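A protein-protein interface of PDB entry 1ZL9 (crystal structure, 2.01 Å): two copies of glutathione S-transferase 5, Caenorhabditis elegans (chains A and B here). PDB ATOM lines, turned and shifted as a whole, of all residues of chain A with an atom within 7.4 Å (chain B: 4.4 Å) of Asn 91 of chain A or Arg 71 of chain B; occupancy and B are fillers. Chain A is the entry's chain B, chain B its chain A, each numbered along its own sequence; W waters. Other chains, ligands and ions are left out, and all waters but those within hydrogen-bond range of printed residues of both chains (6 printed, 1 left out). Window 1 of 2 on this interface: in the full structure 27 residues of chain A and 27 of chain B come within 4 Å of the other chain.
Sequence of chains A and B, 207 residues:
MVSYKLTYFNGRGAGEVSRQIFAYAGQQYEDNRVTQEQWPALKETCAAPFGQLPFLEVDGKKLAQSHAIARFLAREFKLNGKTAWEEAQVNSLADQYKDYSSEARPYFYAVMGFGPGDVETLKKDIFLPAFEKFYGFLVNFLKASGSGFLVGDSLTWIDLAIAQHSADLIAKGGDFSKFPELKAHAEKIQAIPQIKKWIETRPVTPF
The guanidinium group of Arg 71 of chain B lies within hydrogen-bond range of the side-chain amide oxygen of Asn 91 of chain A. The guanidinium group (NH1) of Arg 71 of chain A lies close to the side-chain amide nitrogen (ND2) of Asn 91 of chain B, at 2.8 Å. The guanidinium group (NH1) of Arg 75 of chain B is in salt-bridge range of the side-chain carboxylate (OE1) of Glu 87 of chain A (2.8 Å).
ND2 of Asn 91 of chain A sits close to NH2 of Arg 71 of chain A (3.3 Å). NH2 of Arg 71 of chain B lies within hydrogen-bond range of OD1 of Asn 91 of chain B (3.1 Å). NE of Arg 75 of chain A lies within salt-bridge range of OE1 of Glu 87 of chain A (3.8 Å). NE1 of Trp 85 of chain A sits close to NE2 of Gln 89 of chain A, at 3.5 Å. The side-chain amide nitrogen of Asn 91 of chain A is in hydrogen-bond range of the side-chain carboxylate of Asp 95 of chain A (3.4 Å). The side-chain amide oxygen (OD1) of Asn 80 of chain A lies close to the side-chain carboxylate (OE1) of Glu 87 of chain A.
Ala 68 of chain A touches Asn 91 of chain B. CD of Arg 71 of chain B touches CD of Arg 71 of chain A, at 3.8 Å. Arg 75 of chain A touches Arg 75 of chain B. CE3 of Trp 85 of chain A touches CZ of Phe 72 of chain B, 3.9 Å away. Ala 68 of chain B touches Ala 88 of chain A. Ala 88 of chain A touches Phe 72 of chain B. CA of Ala 68 of chain B touches OD1 of Asn 91 of chain A (3.6 Å). Ser 92 of chain A touches Ala 68 of chain B (N to CB, 3.5 Å). His 67 of chain B touches Asp 95 of chain A (CB to OD2, 3.4 Å). Asp 95 of chain A touches Ala 68 of chain B.
Of the printed residues of chain B, Ala 68 of chain A touches Asn 91. Printed residues of chain B within 4 Å of Arg 75 of chain A: Arg 75. Asn 91 of chain A touches just these residues of chain B: Ala 68 (3.6 Å) and Arg 71 (2.8 Å). Printed residues of chain B within 4 Å of Asp 95 of chain A: His 67 (3.4 Å) and Ala 68 (3.97 Å). Of the printed residues of chain A, Ala 68 of chain B touches Ala 88, Asn 91, Ser 92 and Asp 95. No residue of chain A comes within 4 Å of Ala 70 of chain B. Of chain A, only Arg 71 and Asn 91 come within 4 Å of Arg 71 of chain B. Ala 74 of chain B touches none of the printed residues of chain A. Trp 157 of chain B touches none of the printed residues of chain A. The nearest residue of chain B that does not touch Asn 91 of chain A is His 67 of chain B (4.2 Å). The nearest residue of chain A that does not touch Arg 71 of chain B is Asp 95 of chain A (5.2 Å).
Of the 21 printed residues of chain A, 9 touch a printed residue of chain B. Hydrophobic or aromatic side chains of chain B that line the printed part of chain A: His 67, Ala 68 and Phe 72. Among the printed residues, 13 pairs touch across the chains.
Ala 68 of chain A touches Asn 91 of chain B, and with the chains exchanged Asn 91 of chain A touches Ala 68 of chain B. Arg 71 of chain B touches its own counterpart, Arg 71 of chain A. Arg 71 of chain A touches Asn 91 of chain B, and with the chains exchanged Asn 91 of chain A touches Arg 71 of chain B. Arg 75 of chain B touches its own counterpart, Arg 75 of chain A. Of the 13 pairs that touch across the chains among the printed residues, 6 have their exchanged pair printed and touching as well.
Water W2 lies within hydrogen-bond range of the side-chain carboxylate of Asp 95 of chain A (2.7 Å), the guanidinium group of Arg 71 of chain B (3.0 Å) and the side-chain amide nitrogen of Asn 91 of chain A (3.0 Å). Water W5 lies within hydrogen-bond range of the side-chain carboxylate (OD2) of Asp 95 of chain A (2.8 Å) and the backbone NH (N) of His 67 of chain B (2.9 Å). Water W4 lies within hydrogen-bond range of the guanidinium group of Arg 75 of chain B (3.1 Å) and the guanidinium group of Arg 75 of chain A (3.4 Å).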
ATOM      1  N   HIS A  67       0.460  16.735  -3.957  1.00  0.00           N
ATOM      2  CA  HIS A  67       0.678  17.099  -5.357  1.00  0.00           C
ATOM      3  C   HIS A  67      -0.209  18.312  -5.755  1.00  0.00           C
ATOM      4  O   HIS A  67       0.187  19.107  -6.633  1.00  0.00           O
ATOM      5  CB  HIS A  67       0.363  15.917  -6.301  1.00  0.00           C
ATOM      6  CG  HIS A  67       1.449  14.891  -6.407  1.00  0.00           C
ATOM      7  ND1 HIS A  67       2.525  14.824  -5.556  1.00  0.00           N
ATOM      8  CD2 HIS A  67       1.630  13.893  -7.292  1.00  0.00           C
ATOM      9  CE1 HIS A  67       3.291  13.791  -5.878  1.00  0.00           C
ATOM     10  NE2 HIS A  67       2.756  13.197  -6.919  1.00  0.00           N
ATOM     11  N   ALA A  68      -1.432  18.429  -5.191  1.00  0.00           N
ATOM     12  CA  ALA A  68      -2.243  19.607  -5.481  1.00  0.00           C
ATOM     13  C   ALA A  68      -1.523  20.852  -4.988  1.00  0.00           C
ATOM     14  O   ALA A  68      -1.568  21.896  -5.651  1.00  0.00           O
ATOM     15  CB  ALA A  68      -3.648  19.497  -4.844  1.00  0.00           C
ATOM     16  N   ARG A  71       1.606  21.563  -7.271  1.00  0.00           N
ATOM     17  CA  ARG A  71       1.184  22.093  -8.559  1.00  0.00           C
ATOM     18  C   ARG A  71       0.698  23.533  -8.428  1.00  0.00           C
ATOM     19  O   ARG A  71       0.939  24.351  -9.333  1.00  0.00           O
ATOM     20  CB  ARG A  71       0.092  21.193  -9.187  1.00  0.00           C
ATOM     21  CG  ARG A  71      -0.545  21.753 -10.479  1.00  0.00           C
ATOM     22  CD  ARG A  71      -1.394  20.730 -11.308  1.00  0.00           C
ATOM     23  NE  ARG A  71      -0.537  19.610 -11.697  1.00  0.00           N
ATOM     24  CZ  ARG A  71      -0.406  18.483 -11.040  1.00  0.00           C
ATOM     25  NH1 ARG A  71      -1.181  18.161 -10.031  1.00  0.00           N
ATOM     26  NH2 ARG A  71       0.508  17.628 -11.407  1.00  0.00           N
ATOM     27  N   ARG A  75       2.653  26.487 -10.233  1.00  0.00           N
ATOM     28  CA  ARG A  75       2.062  27.358 -11.241  1.00  0.00           C
ATOM     29  C   ARG A  75       2.214  28.851 -10.866  1.00  0.00           C
ATOM     30  O   ARG A  75       2.504  29.695 -11.730  1.00  0.00           O
ATOM     31  CB  ARG A  75       0.604  27.019 -11.475  1.00  0.00           C
ATOM     32  CG  ARG A  75       0.405  25.700 -12.234  1.00  0.00           C
ATOM     33  CD  ARG A  75      -1.047  25.234 -12.189  1.00  0.00           C
ATOM     34  NE  ARG A  75      -1.844  26.136 -12.979  1.00  0.00           N
ATOM     35  CZ  ARG A  75      -3.125  25.996 -13.272  1.00  0.00           C
ATOM     36  NH1 ARG A  75      -3.832  24.937 -12.839  1.00  0.00           N
ATOM     37  NH2 ARG A  75      -3.682  26.924 -14.049  1.00  0.00           N
ATOM     38  N   ASN A  80       5.784  24.758 -13.173  1.00  0.00           N
ATOM     39  CA  ASN A  80       4.916  23.630 -13.507  1.00  0.00           C
ATOM     40  C   ASN A  80       5.056  23.203 -14.958  1.00  0.00           C
ATOM     41  O   ASN A  80       4.402  22.257 -15.394  1.00  0.00           O
ATOM     42  CB  ASN A  80       3.434  23.957 -13.139  1.00  0.00           C
ATOM     43  CG  ASN A  80       2.514  22.728 -13.180  1.00  0.00           C
ATOM     44  OD1 ASN A  80       1.409  22.746 -13.759  1.00  0.00           O
ATOM     45  ND2 ASN A  80       2.931  21.708 -12.514  1.00  0.00           N
ATOM     46  N   TRP A  85       1.101  21.961 -22.648  1.00  0.00           N
ATOM     47  CA  TRP A  85       1.535  20.605 -22.863  1.00  0.00           C
ATOM     48  C   TRP A  85       2.574  20.164 -21.870  1.00  0.00           C
ATOM     49  O   TRP A  85       2.488  19.037 -21.390  1.00  0.00           O
ATOM     50  CB  TRP A  85       2.049  20.385 -24.280  1.00  0.00           C
ATOM     51  CG  TRP A  85       2.315  18.954 -24.653  1.00  0.00           C
ATOM     52  CD1 TRP A  85       3.531  18.381 -24.925  1.00  0.00           C
ATOM     53  CD2 TRP A  85       1.340  17.931 -24.869  1.00  0.00           C
ATOM     54  NE1 TRP A  85       3.349  17.058 -25.281  1.00  0.00           N
ATOM     55  CE2 TRP A  85       2.015  16.774 -25.270  1.00  0.00           C
ATOM     56  CE3 TRP A  85      -0.052  17.880 -24.771  1.00  0.00           C
ATOM     57  CZ2 TRP A  85       1.351  15.573 -25.531  1.00  0.00           C
ATOM     58  CZ3 TRP A  85      -0.701  16.716 -25.114  1.00  0.00           C
ATOM     59  CH2 TRP A  85       0.010  15.575 -25.462  1.00  0.00           C
ATOM     60  N   GLU A  86       3.579  21.009 -21.587  1.00  0.00           N
ATOM     61  CA  GLU A  86       4.562  20.663 -20.583  1.00  0.00           C
ATOM     62  C   GLU A  86       3.943  20.488 -19.216  1.00  0.00           C
ATOM     63  O   GLU A  86       4.345  19.580 -18.499  1.00  0.00           O
ATOM     64  CB  GLU A  86       5.747  21.627 -20.446  1.00  0.00           C
ATOM     65  CG  GLU A  86       6.609  21.778 -21.684  1.00  0.00           C
ATOM     66  CD  GLU A  86       7.890  22.594 -21.444  1.00  0.00           C
ATOM     67  OE1 GLU A  86       8.137  23.084 -20.317  1.00  0.00           O
ATOM     68  OE2 GLU A  86       8.712  22.676 -22.407  1.00  0.00           O
ATOM     69  N   GLU A  87       2.970  21.330 -18.858  1.00  0.00           N
ATOM     70  CA  GLU A  87       2.276  21.212 -17.549  1.00  0.00           C
ATOM     71  C   GLU A  87       1.633  19.849 -17.435  1.00  0.00           C
ATOM     72  O   GLU A  87       1.658  19.238 -16.368  1.00  0.00           O
ATOM     73  CB  GLU A  87       1.265  22.350 -17.312  1.00  0.00           C
ATOM     74  CG  GLU A  87       1.932  23.727 -17.189  1.00  0.00           C
ATOM     75  CD  GLU A  87       0.983  24.809 -16.703  1.00  0.00           C
ATOM     76  OE1 GLU A  87       0.477  24.719 -15.581  1.00  0.00           O
ATOM     77  OE2 GLU A  87       0.769  25.762 -17.477  1.00  0.00           O
ATOM     78  N   ALA A  88       1.075  19.369 -18.543  1.00  0.00           N
ATOM     79  CA  ALA A  88       0.372  18.125 -18.510  1.00  0.00           C
ATOM     80  C   ALA A  88       1.387  16.949 -18.396  1.00  0.00           C
ATOM     81  O   ALA A  88       1.142  15.980 -17.728  1.00  0.00           O
ATOM     82  CB  ALA A  88      -0.478  18.023 -19.689  1.00  0.00           C
ATOM     83  N   GLN A  89       2.527  17.057 -19.060  1.00  0.00           N
ATOM     84  CA  GLN A  89       3.546  15.995 -18.986  1.00  0.00           C
ATOM     85  C   GLN A  89       4.144  15.926 -17.623  1.00  0.00           C
ATOM     86  O   GLN A  89       4.478  14.826 -17.117  1.00  0.00           O
ATOM     87  CB  GLN A  89       4.640  16.257 -20.041  1.00  0.00           C
ATOM     88  CG  GLN A  89       4.203  16.105 -21.456  1.00  0.00           C
ATOM     89  CD  GLN A  89       3.768  14.685 -21.803  1.00  0.00           C
ATOM     90  OE1 GLN A  89       4.022  13.762 -21.049  1.00  0.00           O
ATOM     91  NE2 GLN A  89       3.054  14.522 -22.903  1.00  0.00           N
ATOM     92  N   VAL A  90       4.336  17.105 -17.006  1.00  0.00           N
ATOM     93  CA  VAL A  90       4.777  17.145 -15.628  1.00  0.00           C
ATOM     94  C   VAL A  90       3.768  16.380 -14.750  1.00  0.00           C
ATOM     95  O   VAL A  90       4.154  15.566 -13.884  1.00  0.00           O
ATOM     96  CB  VAL A  90       5.006  18.606 -15.074  1.00  0.00           C
ATOM     97  CG1 VAL A  90       5.208  18.580 -13.566  1.00  0.00           C
ATOM     98  CG2 VAL A  90       6.269  19.268 -15.738  1.00  0.00           C
ATOM     99  N   ASN A  91       2.473  16.650 -14.960  1.00  0.00           N
ATOM    100  CA  ASN A  91       1.431  15.967 -14.211  1.00  0.00           C
ATOM    101  C   ASN A  91       1.443  14.454 -14.467  1.00  0.00           C
ATOM    102  O   ASN A  91       1.269  13.666 -13.536  1.00  0.00           O
ATOM    103  CB  ASN A  91       0.123  16.574 -14.645  1.00  0.00           C
ATOM    104  CG  ASN A  91      -1.116  16.198 -13.804  1.00  0.00           C
ATOM    105  OD1 ASN A  91      -2.158  16.852 -13.991  1.00  0.00           O
ATOM    106  ND2 ASN A  91      -1.048  15.214 -12.955  1.00  0.00           N
ATOM    107  N   SER A  92       1.684  14.056 -15.719  1.00  0.00           N
ATOM    108  CA  SER A  92       1.707  12.640 -16.094  1.00  0.00           C
ATOM    109  C   SER A  92       2.787  11.894 -15.316  1.00  0.00           C
ATOM    110  O   SER A  92       2.572  10.812 -14.745  1.00  0.00           O
ATOM    111  CB  SER A  92       1.984  12.524 -17.578  1.00  0.00           C
ATOM    112  OG  SER A  92       1.763  11.222 -18.033  1.00  0.00           O
ATOM    113  N   LEU A  93       3.959  12.506 -15.281  1.00  0.00           N
ATOM    114  CA  LEU A  93       5.102  11.876 -14.657  1.00  0.00           C
ATOM    115  C   LEU A  93       4.939  11.843 -13.137  1.00  0.00           C
ATOM    116  O   LEU A  93       5.238  10.839 -12.523  1.00  0.00           O
ATOM    117  CB  LEU A  93       6.371  12.644 -15.047  1.00  0.00           C
ATOM    118  CG  LEU A  93       7.670  11.904 -15.364  1.00  0.00           C
ATOM    119  CD1 LEU A  93       8.937  12.742 -14.989  1.00  0.00           C
ATOM    120  CD2 LEU A  93       7.761  10.412 -15.060  1.00  0.00           C
ATOM    121  N   ALA A  94       4.330  12.891 -12.573  1.00  0.00           N
ATOM    122  CA  ALA A  94       4.125  12.970 -11.149  1.00  0.00           C
ATOM    123  C   ALA A  94       3.114  11.936 -10.725  1.00  0.00           C
ATOM    124  O   ALA A  94       3.261  11.367  -9.666  1.00  0.00           O
ATOM    125  CB  ALA A  94       3.683  14.374 -10.727  1.00  0.00           C
ATOM    126  N   ASP A  95       2.095  11.697 -11.538  1.00  0.00           N
ATOM    127  CA  ASP A  95       1.126  10.665 -11.233  1.00  0.00           C
ATOM    128  C   ASP A  95       1.726   9.276 -11.376  1.00  0.00           C
ATOM    129  O   ASP A  95       1.366   8.377 -10.617  1.00  0.00           O
ATOM    130  CB  ASP A  95      -0.165  10.843 -12.114  1.00  0.00           C
ATOM    131  CG  ASP A  95      -1.062  11.965 -11.605  1.00  0.00           C
ATOM    132  OD1 ASP A  95      -0.640  12.704 -10.625  1.00  0.00           O
ATOM    133  OD2 ASP A  95      -2.236  12.136 -12.059  1.00  0.00           O
ATOM    134  N   GLN A  96       2.633   9.083 -12.343  1.00  0.00           N
ATOM    135  CA  GLN A  96       3.295   7.818 -12.473  1.00  0.00           C
ATOM    136  C   GLN A  96       4.229   7.603 -11.236  1.00  0.00           C
ATOM    137  O   GLN A  96       4.343   6.499 -10.746  1.00  0.00           O
ATOM    138  CB  GLN A  96       4.087   7.714 -13.784  1.00  0.00           C
ATOM    139  CG  GLN A  96       4.683   6.298 -14.018  1.00  0.00           C
ATOM    140  CD  GLN A  96       3.651   5.224 -14.170  1.00  0.00           C
ATOM    141  OE1 GLN A  96       2.561   5.489 -14.708  1.00  0.00           O
ATOM    142  NE2 GLN A  96       3.988   3.974 -13.738  1.00  0.00           N
ATOM    143  N   TYR A  97       4.834   8.684 -10.726  1.00  0.00           N
ATOM    144  CA  TYR A  97       5.640   8.665  -9.501  1.00  0.00           C
ATOM    145  C   TYR A  97       4.778   8.232  -8.308  1.00  0.00           C
ATOM    146  O   TYR A  97       5.216   7.437  -7.485  1.00  0.00           O
ATOM    147  CB  TYR A  97       6.227  10.041  -9.244  1.00  0.00           C
ATOM    148  CG  TYR A  97       7.152  10.163  -8.062  1.00  0.00           C
ATOM    149  CD1 TYR A  97       8.066   9.140  -7.723  1.00  0.00           C
ATOM    150  CD2 TYR A  97       7.174  11.339  -7.296  1.00  0.00           C
ATOM    151  CE1 TYR A  97       8.893   9.284  -6.658  1.00  0.00           C
ATOM    152  CE2 TYR A  97       8.031  11.477  -6.216  1.00  0.00           C
ATOM    153  CZ  TYR A  97       8.884  10.435  -5.905  1.00  0.00           C
ATOM    154  OH  TYR A  97       9.763  10.532  -4.819  1.00  0.00           O
ATOM    155  N   VAL A 151      11.279  17.416 -18.020  1.00  0.00           N
ATOM    156  CA  VAL A 151      10.277  17.923 -18.946  1.00  0.00           C
ATOM    157  C   VAL A 151      10.724  19.257 -19.491  1.00  0.00           C
ATOM    158  O   VAL A 151      10.802  20.230 -18.768  1.00  0.00           O
ATOM    159  CB  VAL A 151       8.903  18.146 -18.262  1.00  0.00           C
ATOM    160  CG1 VAL A 151       7.935  18.830 -19.270  1.00  0.00           C
ATOM    161  CG2 VAL A 151       8.311  16.860 -17.752  1.00  0.00           C
ATOM    162  N   TRP A 157       8.913  21.257 -10.997  1.00  0.00           N
ATOM    163  CA  TRP A 157       8.910  20.673  -9.659  1.00  0.00           C
ATOM    164  C   TRP A 157       9.056  19.162  -9.640  1.00  0.00           C
ATOM    165  O   TRP A 157       9.492  18.616  -8.636  1.00  0.00           O
ATOM    166  CB  TRP A 157       7.657  21.092  -8.887  1.00  0.00           C
ATOM    167  CG  TRP A 157       6.380  20.548  -9.360  1.00  0.00           C
ATOM    168  CD1 TRP A 157       5.520  21.127 -10.238  1.00  0.00           C
ATOM    169  CD2 TRP A 157       5.756  19.328  -8.936  1.00  0.00           C
ATOM    170  NE1 TRP A 157       4.388  20.351 -10.365  1.00  0.00           N
ATOM    171  CE2 TRP A 157       4.500  19.259  -9.562  1.00  0.00           C
ATOM    172  CE3 TRP A 157       6.082  18.343  -7.991  1.00  0.00           C
ATOM    173  CZ2 TRP A 157       3.584  18.209  -9.330  1.00  0.00           C
ATOM    174  CZ3 TRP A 157       5.180  17.277  -7.796  1.00  0.00           C
ATOM    175  CH2 TRP A 157       3.945  17.226  -8.475  1.00  0.00           C
ATOM    176  N   ILE A 158       8.743  18.467 -10.744  1.00  0.00           N
ATOM    177  CA  ILE A 158       9.016  17.031 -10.763  1.00  0.00           C
ATOM    178  C   ILE A 158      10.515  16.703 -10.736  1.00  0.00           C
ATOM    179  O   ILE A 158      10.884  15.686 -10.155  1.00  0.00           O
ATOM    180  CB  ILE A 158       8.287  16.271 -11.913  1.00  0.00           C
ATOM    181  CG1 ILE A 158       8.259  14.756 -11.653  1.00  0.00           C
ATOM    182  CG2 ILE A 158       8.824  16.635 -13.267  1.00  0.00           C
ATOM    183  CD1 ILE A 158       7.661  14.331 -10.363  1.00  0.00           C
ATOM    184  N   HIS B  67      -5.748  11.277 -14.710  1.00  0.00           N
ATOM    185  CA  HIS B  67      -5.938  12.584 -14.108  1.00  0.00           C
ATOM    186  C   HIS B  67      -5.177  13.654 -14.911  1.00  0.00           C
ATOM    187  O   HIS B  67      -5.688  14.761 -15.045  1.00  0.00           O
ATOM    188  CB  HIS B  67      -5.538  12.679 -12.629  1.00  0.00           C
ATOM    189  CG  HIS B  67      -6.482  12.018 -11.666  1.00  0.00           C
ATOM    190  ND1 HIS B  67      -7.570  12.632 -11.150  1.00  0.00           N
ATOM    191  CD2 HIS B  67      -6.371  10.879 -10.959  1.00  0.00           C
ATOM    192  CE1 HIS B  67      -8.227  11.821 -10.346  1.00  0.00           C
ATOM    193  NE2 HIS B  67      -7.525  10.737 -10.219  1.00  0.00           N
ATOM    194  N   ALA B  68      -3.984  13.301 -15.431  1.00  0.00           N
ATOM    195  CA  ALA B  68      -3.230  14.287 -16.214  1.00  0.00           C
ATOM    196  C   ALA B  68      -3.963  14.634 -17.492  1.00  0.00           C
ATOM    197  O   ALA B  68      -4.000  15.780 -17.873  1.00  0.00           O
ATOM    198  CB  ALA B  68      -1.774  13.850 -16.479  1.00  0.00           C
ATOM    199  N   ILE B  69      -4.554  13.639 -18.159  1.00  0.00           N
ATOM    200  CA  ILE B  69      -5.387  13.854 -19.292  1.00  0.00           C
ATOM    201  C   ILE B  69      -6.613  14.701 -18.981  1.00  0.00           C
ATOM    202  O   ILE B  69      -6.871  15.653 -19.682  1.00  0.00           O
ATOM    203  CB  ILE B  69      -5.777  12.510 -19.882  1.00  0.00           C
ATOM    204  CG1 ILE B  69      -4.529  11.747 -20.385  1.00  0.00           C
ATOM    205  CG2 ILE B  69      -6.730  12.661 -21.032  1.00  0.00           C
ATOM    206  CD1 ILE B  69      -4.745  10.268 -20.602  1.00  0.00           C
ATOM    207  N   ALA B  70      -7.380  14.337 -17.951  1.00  0.00           N
ATOM    208  CA  ALA B  70      -8.614  15.046 -17.624  1.00  0.00           C
ATOM    209  C   ALA B  70      -8.285  16.504 -17.300  1.00  0.00           C
ATOM    210  O   ALA B  70      -8.979  17.448 -17.724  1.00  0.00           O
ATOM    211  CB  ALA B  70      -9.278  14.375 -16.410  1.00  0.00           C
ATOM    212  N   ARG B  71      -7.186  16.703 -16.580  1.00  0.00           N
ATOM    213  CA  ARG B  71      -6.783  18.073 -16.189  1.00  0.00           C
ATOM    214  C   ARG B  71      -6.360  18.896 -17.421  1.00  0.00           C
ATOM    215  O   ARG B  71      -6.729  20.059 -17.567  1.00  0.00           O
ATOM    216  CB  ARG B  71      -5.673  18.068 -15.125  1.00  0.00           C
ATOM    217  CG  ARG B  71      -5.225  19.494 -14.678  1.00  0.00           C
ATOM    218  CD  ARG B  71      -4.307  19.554 -13.509  1.00  0.00           C
ATOM    219  NE  ARG B  71      -5.090  19.163 -12.362  1.00  0.00           N
ATOM    220  CZ  ARG B  71      -5.154  17.952 -11.834  1.00  0.00           C
ATOM    221  NH1 ARG B  71      -4.322  16.946 -12.191  1.00  0.00           N
ATOM    222  NH2 ARG B  71      -6.033  17.740 -10.880  1.00  0.00           N
ATOM    223  N   PHE B  72      -5.633  18.276 -18.329  1.00  0.00           N
ATOM    224  CA  PHE B  72      -5.177  18.959 -19.519  1.00  0.00           C
ATOM    225  C   PHE B  72      -6.385  19.377 -20.347  1.00  0.00           C
ATOM    226  O   PHE B  72      -6.536  20.564 -20.729  1.00  0.00           O
ATOM    227  CB  PHE B  72      -4.290  18.030 -20.342  1.00  0.00           C
ATOM    228  CG  PHE B  72      -4.034  18.544 -21.741  1.00  0.00           C
ATOM    229  CD1 PHE B  72      -3.152  19.575 -21.942  1.00  0.00           C
ATOM    230  CD2 PHE B  72      -4.648  17.975 -22.854  1.00  0.00           C
ATOM    231  CE1 PHE B  72      -2.895  20.057 -23.242  1.00  0.00           C
ATOM    232  CE2 PHE B  72      -4.435  18.501 -24.123  1.00  0.00           C
ATOM    233  CZ  PHE B  72      -3.554  19.511 -24.317  1.00  0.00           C
ATOM    234  N   LEU B  73      -7.306  18.422 -20.532  1.00  0.00           N
ATOM    235  CA  LEU B  73      -8.485  18.719 -21.330  1.00  0.00           C
ATOM    236  C   LEU B  73      -9.396  19.725 -20.609  1.00  0.00           C
ATOM    237  O   LEU B  73      -9.925  20.648 -21.246  1.00  0.00           O
ATOM    238  CB  LEU B  73      -9.259  17.465 -21.652  1.00  0.00           C
ATOM    239  CG  LEU B  73      -8.544  16.445 -22.558  1.00  0.00           C
ATOM    240  CD1 LEU B  73      -9.408  15.246 -22.578  1.00  0.00           C
ATOM    241  CD2 LEU B  73      -8.325  16.932 -23.913  1.00  0.00           C
ATOM    242  N   ALA B  74      -9.599  19.557 -19.321  1.00  0.00           N
ATOM    243  CA  ALA B  74     -10.451  20.471 -18.569  1.00  0.00           C
ATOM    244  C   ALA B  74      -9.910  21.911 -18.650  1.00  0.00           C
ATOM    245  O   ALA B  74     -10.716  22.865 -18.784  1.00  0.00           O
ATOM    246  CB  ALA B  74     -10.637  20.043 -17.106  1.00  0.00           C
ATOM    247  N   ARG B  75      -8.596  22.086 -18.562  1.00  0.00           N
ATOM    248  CA  ARG B  75      -8.042  23.427 -18.657  1.00  0.00           C
ATOM    249  C   ARG B  75      -8.253  24.052 -20.039  1.00  0.00           C
ATOM    250  O   ARG B  75      -8.517  25.241 -20.111  1.00  0.00           O
ATOM    251  CB  ARG B  75      -6.588  23.456 -18.317  1.00  0.00           C
ATOM    252  CG  ARG B  75      -6.359  23.280 -16.819  1.00  0.00           C
ATOM    253  CD  ARG B  75      -4.869  23.155 -16.424  1.00  0.00           C
ATOM    254  NE  ARG B  75      -4.094  24.303 -16.829  1.00  0.00           N
ATOM    255  CZ  ARG B  75      -2.794  24.480 -16.593  1.00  0.00           C
ATOM    256  NH1 ARG B  75      -2.076  23.547 -15.941  1.00  0.00           N
ATOM    257  NH2 ARG B  75      -2.220  25.622 -17.004  1.00  0.00           N
ATOM    258  N   ASN B  80     -11.681  23.185 -15.313  1.00  0.00           N
ATOM    259  CA  ASN B  80     -10.768  22.829 -14.226  1.00  0.00           C
ATOM    260  C   ASN B  80     -10.869  23.737 -12.994  1.00  0.00           C
ATOM    261  O   ASN B  80     -10.131  23.550 -12.074  1.00  0.00           O
ATOM    262  CB  ASN B  80      -9.284  22.807 -14.722  1.00  0.00           C
ATOM    263  CG  ASN B  80      -8.334  22.060 -13.742  1.00  0.00           C
ATOM    264  OD1 ASN B  80      -8.639  20.963 -13.344  1.00  0.00           O
ATOM    265  ND2 ASN B  80      -7.135  22.640 -13.440  1.00  0.00           N
ATOM    266  N   ASN B  91      -8.026  19.837  -7.922  1.00  0.00           N
ATOM    267  CA  ASN B  91      -6.899  18.957  -7.848  1.00  0.00           C
ATOM    268  C   ASN B  91      -6.870  18.212  -6.494  1.00  0.00           C
ATOM    269  O   ASN B  91      -6.612  17.022  -6.443  1.00  0.00           O
ATOM    270  CB  ASN B  91      -5.620  19.745  -8.083  1.00  0.00           C
ATOM    271  CG  ASN B  91      -4.391  18.877  -8.356  1.00  0.00           C
ATOM    272  OD1 ASN B  91      -4.389  17.655  -8.227  1.00  0.00           O
ATOM    273  ND2 ASN B  91      -3.364  19.529  -8.845  1.00  0.00           N
ATOM    274  N   TRP B 157     -14.559  19.215 -13.926  1.00  0.00           N
ATOM    275  CA  TRP B 157     -14.421  17.788 -14.295  1.00  0.00           C
ATOM    276  C   TRP B 157     -14.549  16.832 -13.105  1.00  0.00           C
ATOM    277  O   TRP B 157     -14.928  15.672 -13.282  1.00  0.00           O
ATOM    278  CB  TRP B 157     -13.128  17.576 -15.072  1.00  0.00           C
ATOM    279  CG  TRP B 157     -11.843  17.660 -14.341  1.00  0.00           C
ATOM    280  CD1 TRP B 157     -11.039  18.715 -14.225  1.00  0.00           C
ATOM    281  CD2 TRP B 157     -11.156  16.559 -13.698  1.00  0.00           C
ATOM    282  NE1 TRP B 157      -9.910  18.386 -13.496  1.00  0.00           N
ATOM    283  CE2 TRP B 157      -9.958  17.060 -13.167  1.00  0.00           C
ATOM    284  CE3 TRP B 157     -11.455  15.212 -13.514  1.00  0.00           C
ATOM    285  CZ2 TRP B 157      -8.998  16.243 -12.552  1.00  0.00           C
ATOM    286  CZ3 TRP B 157     -10.562  14.429 -12.856  1.00  0.00           C
ATOM    287  CH2 TRP B 157      -9.315  14.933 -12.403  1.00  0.00           C
HETATM  288  O   HOH W   1      -2.197  15.610  -8.662  1.00  0.00           O
HETATM  289  O   HOH W   2      -3.211  14.402 -10.965  1.00  0.00           O
HETATM  290  O   HOH W   3      -2.491  17.764 -16.649  1.00  0.00           O
HETATM  291  O   HOH W   4      -6.061  26.705 -16.514  1.00  0.00           O
HETATM  292  O   HOH W   5      -3.651  10.048 -13.174  1.00  0.00           O
HETATM  293  O   HOH W   6      -3.110  22.097  -7.873  1.00  0.00           O
